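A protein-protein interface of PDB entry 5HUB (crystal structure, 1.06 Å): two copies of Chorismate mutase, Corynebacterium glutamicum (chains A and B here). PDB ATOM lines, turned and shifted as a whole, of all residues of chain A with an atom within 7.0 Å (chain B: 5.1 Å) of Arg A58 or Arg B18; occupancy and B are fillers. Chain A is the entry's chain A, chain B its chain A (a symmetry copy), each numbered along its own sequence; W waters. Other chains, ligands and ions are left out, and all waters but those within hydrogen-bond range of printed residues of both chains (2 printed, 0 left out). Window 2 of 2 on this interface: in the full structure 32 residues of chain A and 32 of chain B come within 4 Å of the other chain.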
ATOM      1  N   ARG A  35       1.144 -29.653  20.326  1.00  0.00           N
ATOM      2  CA  ARG A  35       2.161 -28.936  19.504  1.00  0.00           C
ATOM      3  C   ARG A  35       2.057 -29.367  18.079  1.00  0.00           C
ATOM      4  O   ARG A  35       2.089 -28.456  17.179  1.00  0.00           O
ATOM      5  CB  ARG A  35       3.559 -29.342  20.062  1.00  0.00           C
ATOM      6  CG  ARG A  35       4.663 -28.456  19.487  1.00  0.00           C
ATOM      7  CD  ARG A  35       5.959 -29.223  19.477  1.00  0.00           C
ATOM      8  NE  ARG A  35       7.067 -28.339  19.231  1.00  0.00           N
ATOM      9  CZ  ARG A  35       7.419 -27.887  18.030  1.00  0.00           C
ATOM     10  NH1 ARG A  35       8.394 -26.982  17.949  1.00  0.00           N
ATOM     11  NH2 ARG A  35       6.804 -28.324  16.947  1.00  0.00           N
ATOM     12  N   ILE A  38      -1.127 -27.956  16.295  1.00  0.00           N
ATOM     13  CA  ILE A  38      -0.959 -26.514  15.989  1.00  0.00           C
ATOM     14  C   ILE A  38       0.022 -26.364  14.855  1.00  0.00           C
ATOM     15  O   ILE A  38      -0.247 -25.564  13.900  1.00  0.00           O
ATOM     16  CB  ILE A  38      -0.452 -25.751  17.194  1.00  0.00           C
ATOM     17  CG1 ILE A  38      -1.503 -25.715  18.260  1.00  0.00           C
ATOM     18  CG2 ILE A  38      -0.104 -24.293  16.795  1.00  0.00           C
ATOM     19  CD1 ILE A  38      -1.040 -25.270  19.614  1.00  0.00           C
ATOM     20  N   SER A  39       1.156 -26.991  14.883  1.00  0.00           N
ATOM     21  CA  SER A  39       2.131 -26.878  13.852  1.00  0.00           C
ATOM     22  C   SER A  39       1.582 -27.251  12.504  1.00  0.00           C
ATOM     23  O   SER A  39       1.776 -26.491  11.528  1.00  0.00           O
ATOM     24  CB  SER A  39       3.379 -27.675  14.206  1.00  0.00           C
ATOM     25  OG  SER A  39       4.379 -27.389  13.247  1.00  0.00           O
ATOM     26  N   ILE A  42      -0.636 -24.536  10.978  1.00  0.00           N
ATOM     27  CA  ILE A  42       0.037 -23.261  10.599  1.00  0.00           C
ATOM     28  C   ILE A  42       1.198 -23.291   9.559  1.00  0.00           C
ATOM     29  O   ILE A  42       1.658 -22.248   9.063  1.00  0.00           O
ATOM     30  CB  ILE A  42       0.541 -22.451  11.855  1.00  0.00           C
ATOM     31  CG1 ILE A  42       1.825 -22.963  12.495  1.00  0.00           C
ATOM     32  CG2 ILE A  42      -0.551 -22.299  12.871  1.00  0.00           C
ATOM     33  CD1 ILE A  42       2.324 -22.076  13.602  1.00  0.00           C
ATOM     34  N   GLY A  43       1.705 -24.494   9.290  1.00  0.00           N
ATOM     35  CA  GLY A  43       2.926 -24.684   8.514  1.00  0.00           C
ATOM     36  C   GLY A  43       2.692 -24.160   7.129  1.00  0.00           C
ATOM     37  O   GLY A  43       1.673 -24.513   6.509  1.00  0.00           O
ATOM     38  N   LYS A  44       3.618 -23.314   6.660  1.00  0.00           N
ATOM     39  CA  LYS A  44       3.389 -22.527   5.457  1.00  0.00           C
ATOM     40  C   LYS A  44       3.366 -23.356   4.175  1.00  0.00           C
ATOM     41  O   LYS A  44       4.042 -24.391   3.985  1.00  0.00           O
ATOM     42  CB  LYS A  44       4.363 -21.331   5.288  1.00  0.00           C
ATOM     43  CG  LYS A  44       3.694 -20.025   4.823  1.00  0.00           C
ATOM     44  CD  LYS A  44       4.635 -19.086   4.082  1.00  0.00           C
ATOM     45  CE  LYS A  44       4.092 -17.650   4.066  1.00  0.00           C
ATOM     46  NZ  LYS A  44       4.108 -16.968   2.732  1.00  0.00           N
ATOM     47  N   MET A  47       6.653 -21.927  -0.359  1.00  0.00           N
ATOM     48  CA  MET A  47       7.710 -21.039   0.148  1.00  0.00           C
ATOM     49  C   MET A  47       8.712 -20.611  -0.935  1.00  0.00           C
ATOM     50  O   MET A  47       9.000 -21.331  -1.857  1.00  0.00           O
ATOM     51  CB  MET A  47       8.451 -21.687   1.336  1.00  0.00           C
ATOM     52  CG  MET A  47       7.599 -21.948   2.629  1.00  0.00           C
ATOM     53  SD  MET A  47       8.580 -21.827   4.098  1.00  0.00           S
ATOM     54  CE  MET A  47       9.335 -23.458   4.118  1.00  0.00           C
ATOM     55  N   GLY A  51      11.912 -17.331   2.146  1.00  0.00           N
ATOM     56  CA  GLY A  51      11.024 -17.757   3.201  1.00  0.00           C
ATOM     57  C   GLY A  51      11.559 -19.025   3.884  1.00  0.00           C
ATOM     58  O   GLY A  51      11.420 -19.194   5.109  1.00  0.00           O
ATOM     59  N   THR A  52      12.178 -19.892   3.107  1.00  0.00           N
ATOM     60  CA  THR A  52      12.704 -21.153   3.620  1.00  0.00           C
ATOM     61  C   THR A  52      13.902 -20.815   4.529  1.00  0.00           C
ATOM     62  O   THR A  52      14.158 -21.495   5.559  1.00  0.00           O
ATOM     63  CB  THR A  52      12.963 -22.042   2.388  1.00  0.00           C
ATOM     64  OG1 THR A  52      11.703 -22.313   1.745  1.00  0.00           O
ATOM     65  CG2 THR A  52      13.560 -23.351   2.788  1.00  0.00           C
ATOM     66  N   ARG A  53      14.638 -19.769   4.228  1.00  0.00           N
ATOM     67  CA  ARG A  53      15.727 -19.318   5.053  1.00  0.00           C
ATOM     68  C   ARG A  53      15.265 -18.841   6.483  1.00  0.00           C
ATOM     69  O   ARG A  53      15.932 -19.150   7.498  1.00  0.00           O
ATOM     70  CB  ARG A  53      16.462 -18.276   4.229  1.00  0.00           C
ATOM     71  CG  ARG A  53      17.482 -17.538   4.990  1.00  0.00           C
ATOM     72  CD  ARG A  53      18.014 -16.437   4.070  1.00  0.00           C
ATOM     73  NE  ARG A  53      19.025 -15.686   4.729  1.00  0.00           N
ATOM     74  CZ  ARG A  53      19.649 -14.646   4.244  1.00  0.00           C
ATOM     75  NH1 ARG A  53      20.548 -14.069   4.985  1.00  0.00           N
ATOM     76  NH2 ARG A  53      19.331 -14.141   3.056  1.00  0.00           N
ATOM     77  N   LEU A  54      14.130 -18.142   6.575  1.00  0.00           N
ATOM     78  CA  LEU A  54      13.561 -17.718   7.809  1.00  0.00           C
ATOM     79  C   LEU A  54      13.152 -18.950   8.675  1.00  0.00           C
ATOM     80  O   LEU A  54      13.371 -18.972   9.866  1.00  0.00           O
ATOM     81  CB  LEU A  54      12.356 -16.825   7.539  1.00  0.00           C
ATOM     82  CG  LEU A  54      12.621 -15.469   6.844  1.00  0.00           C
ATOM     83  CD1 LEU A  54      11.330 -14.780   6.428  1.00  0.00           C
ATOM     84  CD2 LEU A  54      13.369 -14.602   7.810  1.00  0.00           C
ATOM     85  N   VAL A  55      12.554 -19.937   8.056  1.00  0.00           N
ATOM     86  CA  VAL A  55      12.166 -21.147   8.716  1.00  0.00           C
ATOM     87  C   VAL A  55      13.384 -21.863   9.244  1.00  0.00           C
ATOM     88  O   VAL A  55      13.391 -22.355  10.394  1.00  0.00           O
ATOM     89  CB  VAL A  55      11.334 -22.056   7.798  1.00  0.00           C
ATOM     90  CG1 VAL A  55      11.121 -23.405   8.402  1.00  0.00           C
ATOM     91  CG2 VAL A  55      10.000 -21.396   7.490  1.00  0.00           C
ATOM     92  N   HIS A  56      14.423 -21.963   8.456  1.00  0.00           N
ATOM     93  CA  HIS A  56      15.639 -22.656   8.896  1.00  0.00           C
ATOM     94  C   HIS A  56      16.204 -22.007  10.108  1.00  0.00           C
ATOM     95  O   HIS A  56      16.593 -22.695  11.097  1.00  0.00           O
ATOM     96  CB  HIS A  56      16.675 -22.707   7.767  1.00  0.00           C
ATOM     97  CG  HIS A  56      17.977 -23.248   8.176  1.00  0.00           C
ATOM     98  ND1 HIS A  56      18.169 -24.597   8.359  1.00  0.00           N
ATOM     99  CD2 HIS A  56      19.131 -22.649   8.530  1.00  0.00           C
ATOM    100  CE1 HIS A  56      19.406 -24.802   8.763  1.00  0.00           C
ATOM    101  NE2 HIS A  56      20.014 -23.636   8.875  1.00  0.00           N
ATOM    102  N   THR A  57      16.265 -20.674  10.125  1.00  0.00           N
ATOM    103  CA  THR A  57      16.797 -19.959  11.274  1.00  0.00           C
ATOM    104  C   THR A  57      15.943 -20.230  12.530  1.00  0.00           C
ATOM    105  O   THR A  57      16.525 -20.417  13.621  1.00  0.00           O
ATOM    106  CB  THR A  57      16.913 -18.426  10.939  1.00  0.00           C
ATOM    107  OG1 THR A  57      17.695 -18.288   9.765  1.00  0.00           O
ATOM    108  CG2 THR A  57      17.515 -17.657  12.041  1.00  0.00           C
ATOM    109  N   ARG A  58      14.638 -20.290  12.383  1.00  0.00           N
ATOM    110  CA  ARG A  58      13.801 -20.634  13.522  1.00  0.00           C
ATOM    111  C   ARG A  58      14.067 -22.088  13.980  1.00  0.00           C
ATOM    112  O   ARG A  58      14.019 -22.340  15.195  1.00  0.00           O
ATOM    113  CB  ARG A  58      12.331 -20.504  13.166  1.00  0.00           C
ATOM    114  CG  ARG A  58      11.859 -19.066  13.052  1.00  0.00           C
ATOM    115  CD  ARG A  58      10.348 -18.887  13.242  1.00  0.00           C
ATOM    116  NE  ARG A  58       9.564 -19.762  12.403  1.00  0.00           N
ATOM    117  CZ  ARG A  58       9.029 -19.475  11.231  1.00  0.00           C
ATOM    118  NH1 ARG A  58       9.154 -18.264  10.721  1.00  0.00           N
ATOM    119  NH2 ARG A  58       8.353 -20.409  10.571  1.00  0.00           N
ATOM    120  N   GLU A  59      14.256 -23.017  13.072  1.00  0.00           N
ATOM    121  CA  GLU A  59      14.475 -24.433  13.443  1.00  0.00           C
ATOM    122  C   GLU A  59      15.780 -24.531  14.153  1.00  0.00           C
ATOM    123  O   GLU A  59      15.854 -25.306  15.147  1.00  0.00           O
ATOM    124  CB  GLU A  59      14.410 -25.284  12.192  1.00  0.00           C
ATOM    125  CG  GLU A  59      13.031 -25.456  11.563  1.00  0.00           C
ATOM    126  CD  GLU A  59      13.010 -26.325  10.294  1.00  0.00           C
ATOM    127  OE1 GLU A  59      14.076 -26.619   9.756  1.00  0.00           O
ATOM    128  OE2 GLU A  59      11.914 -26.712   9.886  1.00  0.00           O
ATOM    129  N   VAL A  60      16.828 -23.839  13.746  1.00  0.00           N
ATOM    130  CA  VAL A  60      18.086 -23.865  14.473  1.00  0.00           C
ATOM    131  C   VAL A  60      17.954 -23.352  15.884  1.00  0.00           C
ATOM    132  O   VAL A  60      18.541 -23.929  16.817  1.00  0.00           O
ATOM    133  CB  VAL A  60      19.173 -23.106  13.678  1.00  0.00           C
ATOM    134  CG1 VAL A  60      20.422 -22.947  14.554  1.00  0.00           C
ATOM    135  CG2 VAL A  60      19.474 -23.878  12.402  1.00  0.00           C
ATOM    136  N   ALA A  61      17.189 -22.291  16.109  1.00  0.00           N
ATOM    137  CA  ALA A  61      16.966 -21.800  17.465  1.00  0.00           C
ATOM    138  C   ALA A  61      16.326 -22.892  18.342  1.00  0.00           C
ATOM    139  O   ALA A  61      16.637 -22.986  19.527  1.00  0.00           O
ATOM    140  CB  ALA A  61      16.033 -20.609  17.422  1.00  0.00           C
ATOM    141  N   ILE A  62      15.361 -23.594  17.799  1.00  0.00           N
ATOM    142  CA  ILE A  62      14.645 -24.627  18.545  1.00  0.00           C
ATOM    143  C   ILE A  62      15.648 -25.742  18.886  1.00  0.00           C
ATOM    144  O   ILE A  62      15.698 -26.221  20.033  1.00  0.00           O
ATOM    145  CB  ILE A  62      13.436 -25.165  17.747  1.00  0.00           C
ATOM    146  CG1 ILE A  62      12.396 -24.026  17.617  1.00  0.00           C
ATOM    147  CG2 ILE A  62      12.880 -26.443  18.442  1.00  0.00           C
ATOM    148  CD1 ILE A  62      11.270 -24.350  16.682  1.00  0.00           C
ATOM    149  N   ILE A  63      16.415 -26.197  17.931  1.00  0.00           N
ATOM    150  CA  ILE A  63      17.417 -27.244  18.147  1.00  0.00           C
ATOM    151  C   ILE A  63      18.390 -26.812  19.228  1.00  0.00           C
ATOM    152  O   ILE A  63      18.706 -27.544  20.152  1.00  0.00           O
ATOM    153  CB  ILE A  63      18.111 -27.629  16.811  1.00  0.00           C
ATOM    154  CG1 ILE A  63      17.113 -28.315  15.890  1.00  0.00           C
ATOM    155  CG2 ILE A  63      19.363 -28.435  17.060  1.00  0.00           C
ATOM    156  CD1 ILE A  63      17.510 -28.353  14.410  1.00  0.00           C
ATOM    157  N   LEU A  82       9.964 -31.316  15.019  1.00  0.00           N
ATOM    158  CA  LEU A  82       9.953 -30.632  13.719  1.00  0.00           C
ATOM    159  C   LEU A  82       9.422 -31.521  12.635  1.00  0.00           C
ATOM    160  O   LEU A  82       8.606 -31.050  11.812  1.00  0.00           O
ATOM    161  CB  LEU A  82      11.340 -30.110  13.396  1.00  0.00           C
ATOM    162  CG  LEU A  82      11.845 -28.998  14.315  1.00  0.00           C
ATOM    163  CD1 LEU A  82      13.276 -28.618  13.937  1.00  0.00           C
ATOM    164  CD2 LEU A  82      10.939 -27.746  14.231  1.00  0.00           C
ATOM    165  N   GLY A  85       5.663 -31.877  13.017  1.00  0.00           N
ATOM    166  CA  GLY A  85       4.932 -30.622  12.821  1.00  0.00           C
ATOM    167  C   GLY A  85       4.777 -30.226  11.383  1.00  0.00           C
ATOM    168  O   GLY A  85       4.162 -29.197  11.151  1.00  0.00           O
ATOM    169  N   ILE B  14      -1.449 -16.852  13.006  1.00  0.00           N
ATOM    170  CA  ILE B  14      -0.180 -17.635  13.002  1.00  0.00           C
ATOM    171  C   ILE B  14       0.718 -17.209  14.137  1.00  0.00           C
ATOM    172  O   ILE B  14       1.304 -18.101  14.817  1.00  0.00           O
ATOM    173  CB  ILE B  14       0.522 -17.490  11.635  1.00  0.00           C
ATOM    174  CG1 ILE B  14      -0.308 -18.130  10.538  1.00  0.00           C
ATOM    175  CG2 ILE B  14       1.917 -18.087  11.668  1.00  0.00           C
ATOM    176  CD1 ILE B  14       0.060 -17.690   9.134  1.00  0.00           C
ATOM    177  N   GLN B  15       0.798 -15.930  14.437  1.00  0.00           N
ATOM    178  CA  GLN B  15       1.482 -15.324  15.561  1.00  0.00           C
ATOM    179  C   GLN B  15       1.141 -16.011  16.865  1.00  0.00           C
ATOM    180  O   GLN B  15       2.001 -16.414  17.750  1.00  0.00           O
ATOM    181  CB  GLN B  15       1.040 -13.829  15.637  1.00  0.00           C
ATOM    182  CG  GLN B  15       1.699 -13.140  16.808  1.00  0.00           C
ATOM    183  CD  GLN B  15       3.178 -13.061  16.600  1.00  0.00           C
ATOM    184  OE1 GLN B  15       3.601 -12.808  15.463  1.00  0.00           O
ATOM    185  NE2 GLN B  15       3.963 -13.132  17.663  1.00  0.00           N
ATOM    186  N   LYS B  16      -0.153 -16.051  17.091  1.00  0.00           N
ATOM    187  CA  LYS B  16      -0.671 -16.578  18.349  1.00  0.00           C
ATOM    188  C   LYS B  16      -0.317 -18.052  18.454  1.00  0.00           C
ATOM    189  O   LYS B  16       0.080 -18.529  19.549  1.00  0.00           O
ATOM    190  CB  LYS B  16      -2.171 -16.356  18.404  1.00  0.00           C
ATOM    191  CG  LYS B  16      -2.810 -16.581  19.734  1.00  0.00           C
ATOM    192  CD  LYS B  16      -3.845 -15.593  20.166  1.00  0.00           C
ATOM    193  CE  LYS B  16      -4.082 -15.743  21.649  1.00  0.00           C
ATOM    194  NZ  LYS B  16      -3.023 -15.188  22.531  1.00  0.00           N
ATOM    195  N   TYR B  17      -0.452 -18.800  17.366  1.00  0.00           N
ATOM    196  CA  TYR B  17      -0.075 -20.218  17.365  1.00  0.00           C
ATOM    197  C   TYR B  17       1.429 -20.385  17.568  1.00  0.00           C
ATOM    198  O   TYR B  17       1.828 -21.386  18.283  1.00  0.00           O
ATOM    199  CB  TYR B  17      -0.540 -20.888  16.076  1.00  0.00           C
ATOM    200  CG  TYR B  17      -2.011 -21.172  15.967  1.00  0.00           C
ATOM    201  CD1 TYR B  17      -2.711 -21.796  17.013  1.00  0.00           C
ATOM    202  CD2 TYR B  17      -2.715 -20.922  14.783  1.00  0.00           C
ATOM    203  CE1 TYR B  17      -4.064 -22.099  16.894  1.00  0.00           C
ATOM    204  CE2 TYR B  17      -4.062 -21.227  14.666  1.00  0.00           C
ATOM    205  CZ  TYR B  17      -4.733 -21.807  15.725  1.00  0.00           C
ATOM    206  OH  TYR B  17      -6.080 -22.116  15.610  1.00  0.00           O
ATOM    207  N   ARG B  18       2.310 -19.565  17.021  1.00  0.00           N
ATOM    208  CA  ARG B  18       3.732 -19.710  17.257  1.00  0.00           C
ATOM    209  C   ARG B  18       4.061 -19.463  18.706  1.00  0.00           C
ATOM    210  O   ARG B  18       4.924 -20.173  19.281  1.00  0.00           O
ATOM    211  CB  ARG B  18       4.542 -18.765  16.369  1.00  0.00           C
ATOM    212  CG  ARG B  18       4.452 -19.096  14.904  1.00  0.00           C
ATOM    213  CD  ARG B  18       5.534 -20.051  14.447  1.00  0.00           C
ATOM    214  NE  ARG B  18       5.374 -20.343  13.017  1.00  0.00           N
ATOM    215  CZ  ARG B  18       5.358 -21.548  12.447  1.00  0.00           C
ATOM    216  NH1 ARG B  18       5.158 -21.613  11.140  1.00  0.00           N
ATOM    217  NH2 ARG B  18       5.535 -22.681  13.135  1.00  0.00           N
ATOM    218  N   GLU B  19       3.371 -18.522  19.328  1.00  0.00           N
ATOM    219  CA  GLU B  19       3.492 -18.250  20.763  1.00  0.00           C
ATOM    220  C   GLU B  19       3.111 -19.497  21.583  1.00  0.00           C
ATOM    221  O   GLU B  19       3.770 -19.846  22.563  1.00  0.00           O
ATOM    222  CB  GLU B  19       2.580 -17.029  21.144  1.00  0.00           C
ATOM    223  CG  GLU B  19       3.020 -15.652  20.688  1.00  0.00           C
ATOM    224  CD  GLU B  19       1.967 -14.559  20.780  1.00  0.00           C
ATOM    225  OE1 GLU B  19       0.864 -14.638  21.385  1.00  0.00           O
ATOM    226  OE2 GLU B  19       2.385 -13.570  20.168  1.00  0.00           O
ATOM    227  N   GLU B  20       2.013 -20.084  21.208  1.00  0.00           N
ATOM    228  CA  GLU B  20       1.592 -21.319  21.909  1.00  0.00           C
ATOM    229  C   GLU B  20       2.615 -22.395  21.698  1.00  0.00           C
ATOM    230  O   GLU B  20       2.881 -23.177  22.669  1.00  0.00           O
ATOM    231  CB  GLU B  20       0.259 -21.765  21.383  1.00  0.00           C
ATOM    232  CG  GLU B  20      -0.304 -22.771  22.389  1.00  0.00           C
ATOM    233  CD  GLU B  20      -1.745 -23.180  22.261  1.00  0.00           C
ATOM    234  OE1 GLU B  20      -2.422 -22.619  21.376  1.00  0.00           O
ATOM    235  OE2 GLU B  20      -2.187 -24.010  23.068  1.00  0.00           O
ATOM    236  N   ILE B  21       3.167 -22.635  20.545  1.00  0.00           N
ATOM    237  CA  ILE B  21       4.225 -23.649  20.366  1.00  0.00           C
ATOM    238  C   ILE B  21       5.412 -23.321  21.230  1.00  0.00           C
ATOM    239  O   ILE B  21       5.961 -24.265  21.844  1.00  0.00           O
ATOM    240  CB  ILE B  21       4.576 -23.805  18.869  1.00  0.00           C
ATOM    241  CG1 ILE B  21       3.423 -24.422  18.117  1.00  0.00           C
ATOM    242  CG2 ILE B  21       5.875 -24.573  18.678  1.00  0.00           C
ATOM    243  CD1 ILE B  21       3.577 -24.313  16.600  1.00  0.00           C
ATOM    244  N   ASN B  22       5.843 -22.063  21.367  1.00  0.00           N
ATOM    245  CA  ASN B  22       6.900 -21.710  22.303  1.00  0.00           C
ATOM    246  C   ASN B  22       6.586 -22.223  23.731  1.00  0.00           C
ATOM    247  O   ASN B  22       7.453 -22.775  24.419  1.00  0.00           O
ATOM    248  CB  ASN B  22       7.113 -20.160  22.326  1.00  0.00           C
ATOM    249  CG  ASN B  22       7.698 -19.560  21.017  1.00  0.00           C
ATOM    250  OD1 ASN B  22       8.161 -20.240  20.157  1.00  0.00           O
ATOM    251  ND2 ASN B  22       7.609 -18.216  20.892  1.00  0.00           N
HETATM  252  O   HOH W   1       4.520 -25.089  11.191  1.00  0.00           O
HETATM  253  O   HOH W   2       3.782 -19.902   9.079  1.00  0.00           O
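NH2 of Arg A58 sits close to NH1 of Arg B18 (3.5 Å).
Arg A58 touches just one residue of chain B: Arg B18. Of chain A, only Ile A42 and Arg A58 come within 4 Å of Arg B18. Of the printed residues of chain B, Arg A35 touches Ile B21 (3.6 Å). Printed residues of chain A within 4 Å of Ile B21: Arg A35 (3.6 Å), Ile A38 (3.7 Å), Ser A39 (3.998 Å) and Ile A42 (3.9 Å). Of the printed residues of chain A, Tyr B17 touches Ile A38 and Ile A42. Of the printed residues of chain A, Glu B20 touches Ile A38. Printed residues of chain B within 4 Å of Ser A39: Ile B21 (3.998 Å). Glu A59 touches none of the printed residues of chain B. The nearest printed residue of chain B that does not touch Arg A58 is Ile B14 (6.9 Å). The nearest residue of chain A that does not touch Arg B18 is Gly A43 (4.6 Å).
No position is printed for both chains.
The side-chain hydroxyl (OG) of Ser A39 sits at hydrogen-bond distance from the backbone carbonyl oxygen (O) of Gly A85, 2.8 Å away. O of Arg B18 sits close to OD1 of Asn B22 (3.4 Å).
Of the 9 printed residues of chain B, 4 touch a printed residue of chain A. Hydrophobic or aromatic side chains of chain B that line the printed part of chain A: Tyr B17 and Ile B21. Printed residues of chain A that touch a printed residue of chain B: Arg A35, Ile A38, Ser A39, Ile A42 and Arg A58. Hydrophobic or aromatic side chains of chain A that line the printed part of chain B: Ile A38 and Ile A42. Among the printed residues, no Asp or Glu carboxylate lies within 4 Å of a Lys or Arg side-chain nitrogen of the other chain.
Among the printed residues, pairs that only touch across the chains: Arg A35 with Ile B21 (3.6 Å), Ile A38 with Tyr B17 (3.5 Å), Ile A38 with Glu B20 (3.4 Å), Ile A38 with Ile B21 (3.7 Å), Ser A39 with Ile B21 (3.998 Å), Ile A42 with Tyr B17 (3.2 Å), Ile A42 with Arg B18 (3.3 Å) and Ile A42 with Ile B21 (3.9 Å).
Water W2 lies within hydrogen-bond range of the guanidinium group (NH1) of Arg B18 and the backbone carbonyl oxygen (O) of Ile A42. Water W1 lies within hydrogen-bond range of OG of Ser A39 (3.1 Å), NH2 of Arg B18 (3.3 Å) and N of Gly A43 (3.4 Å).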
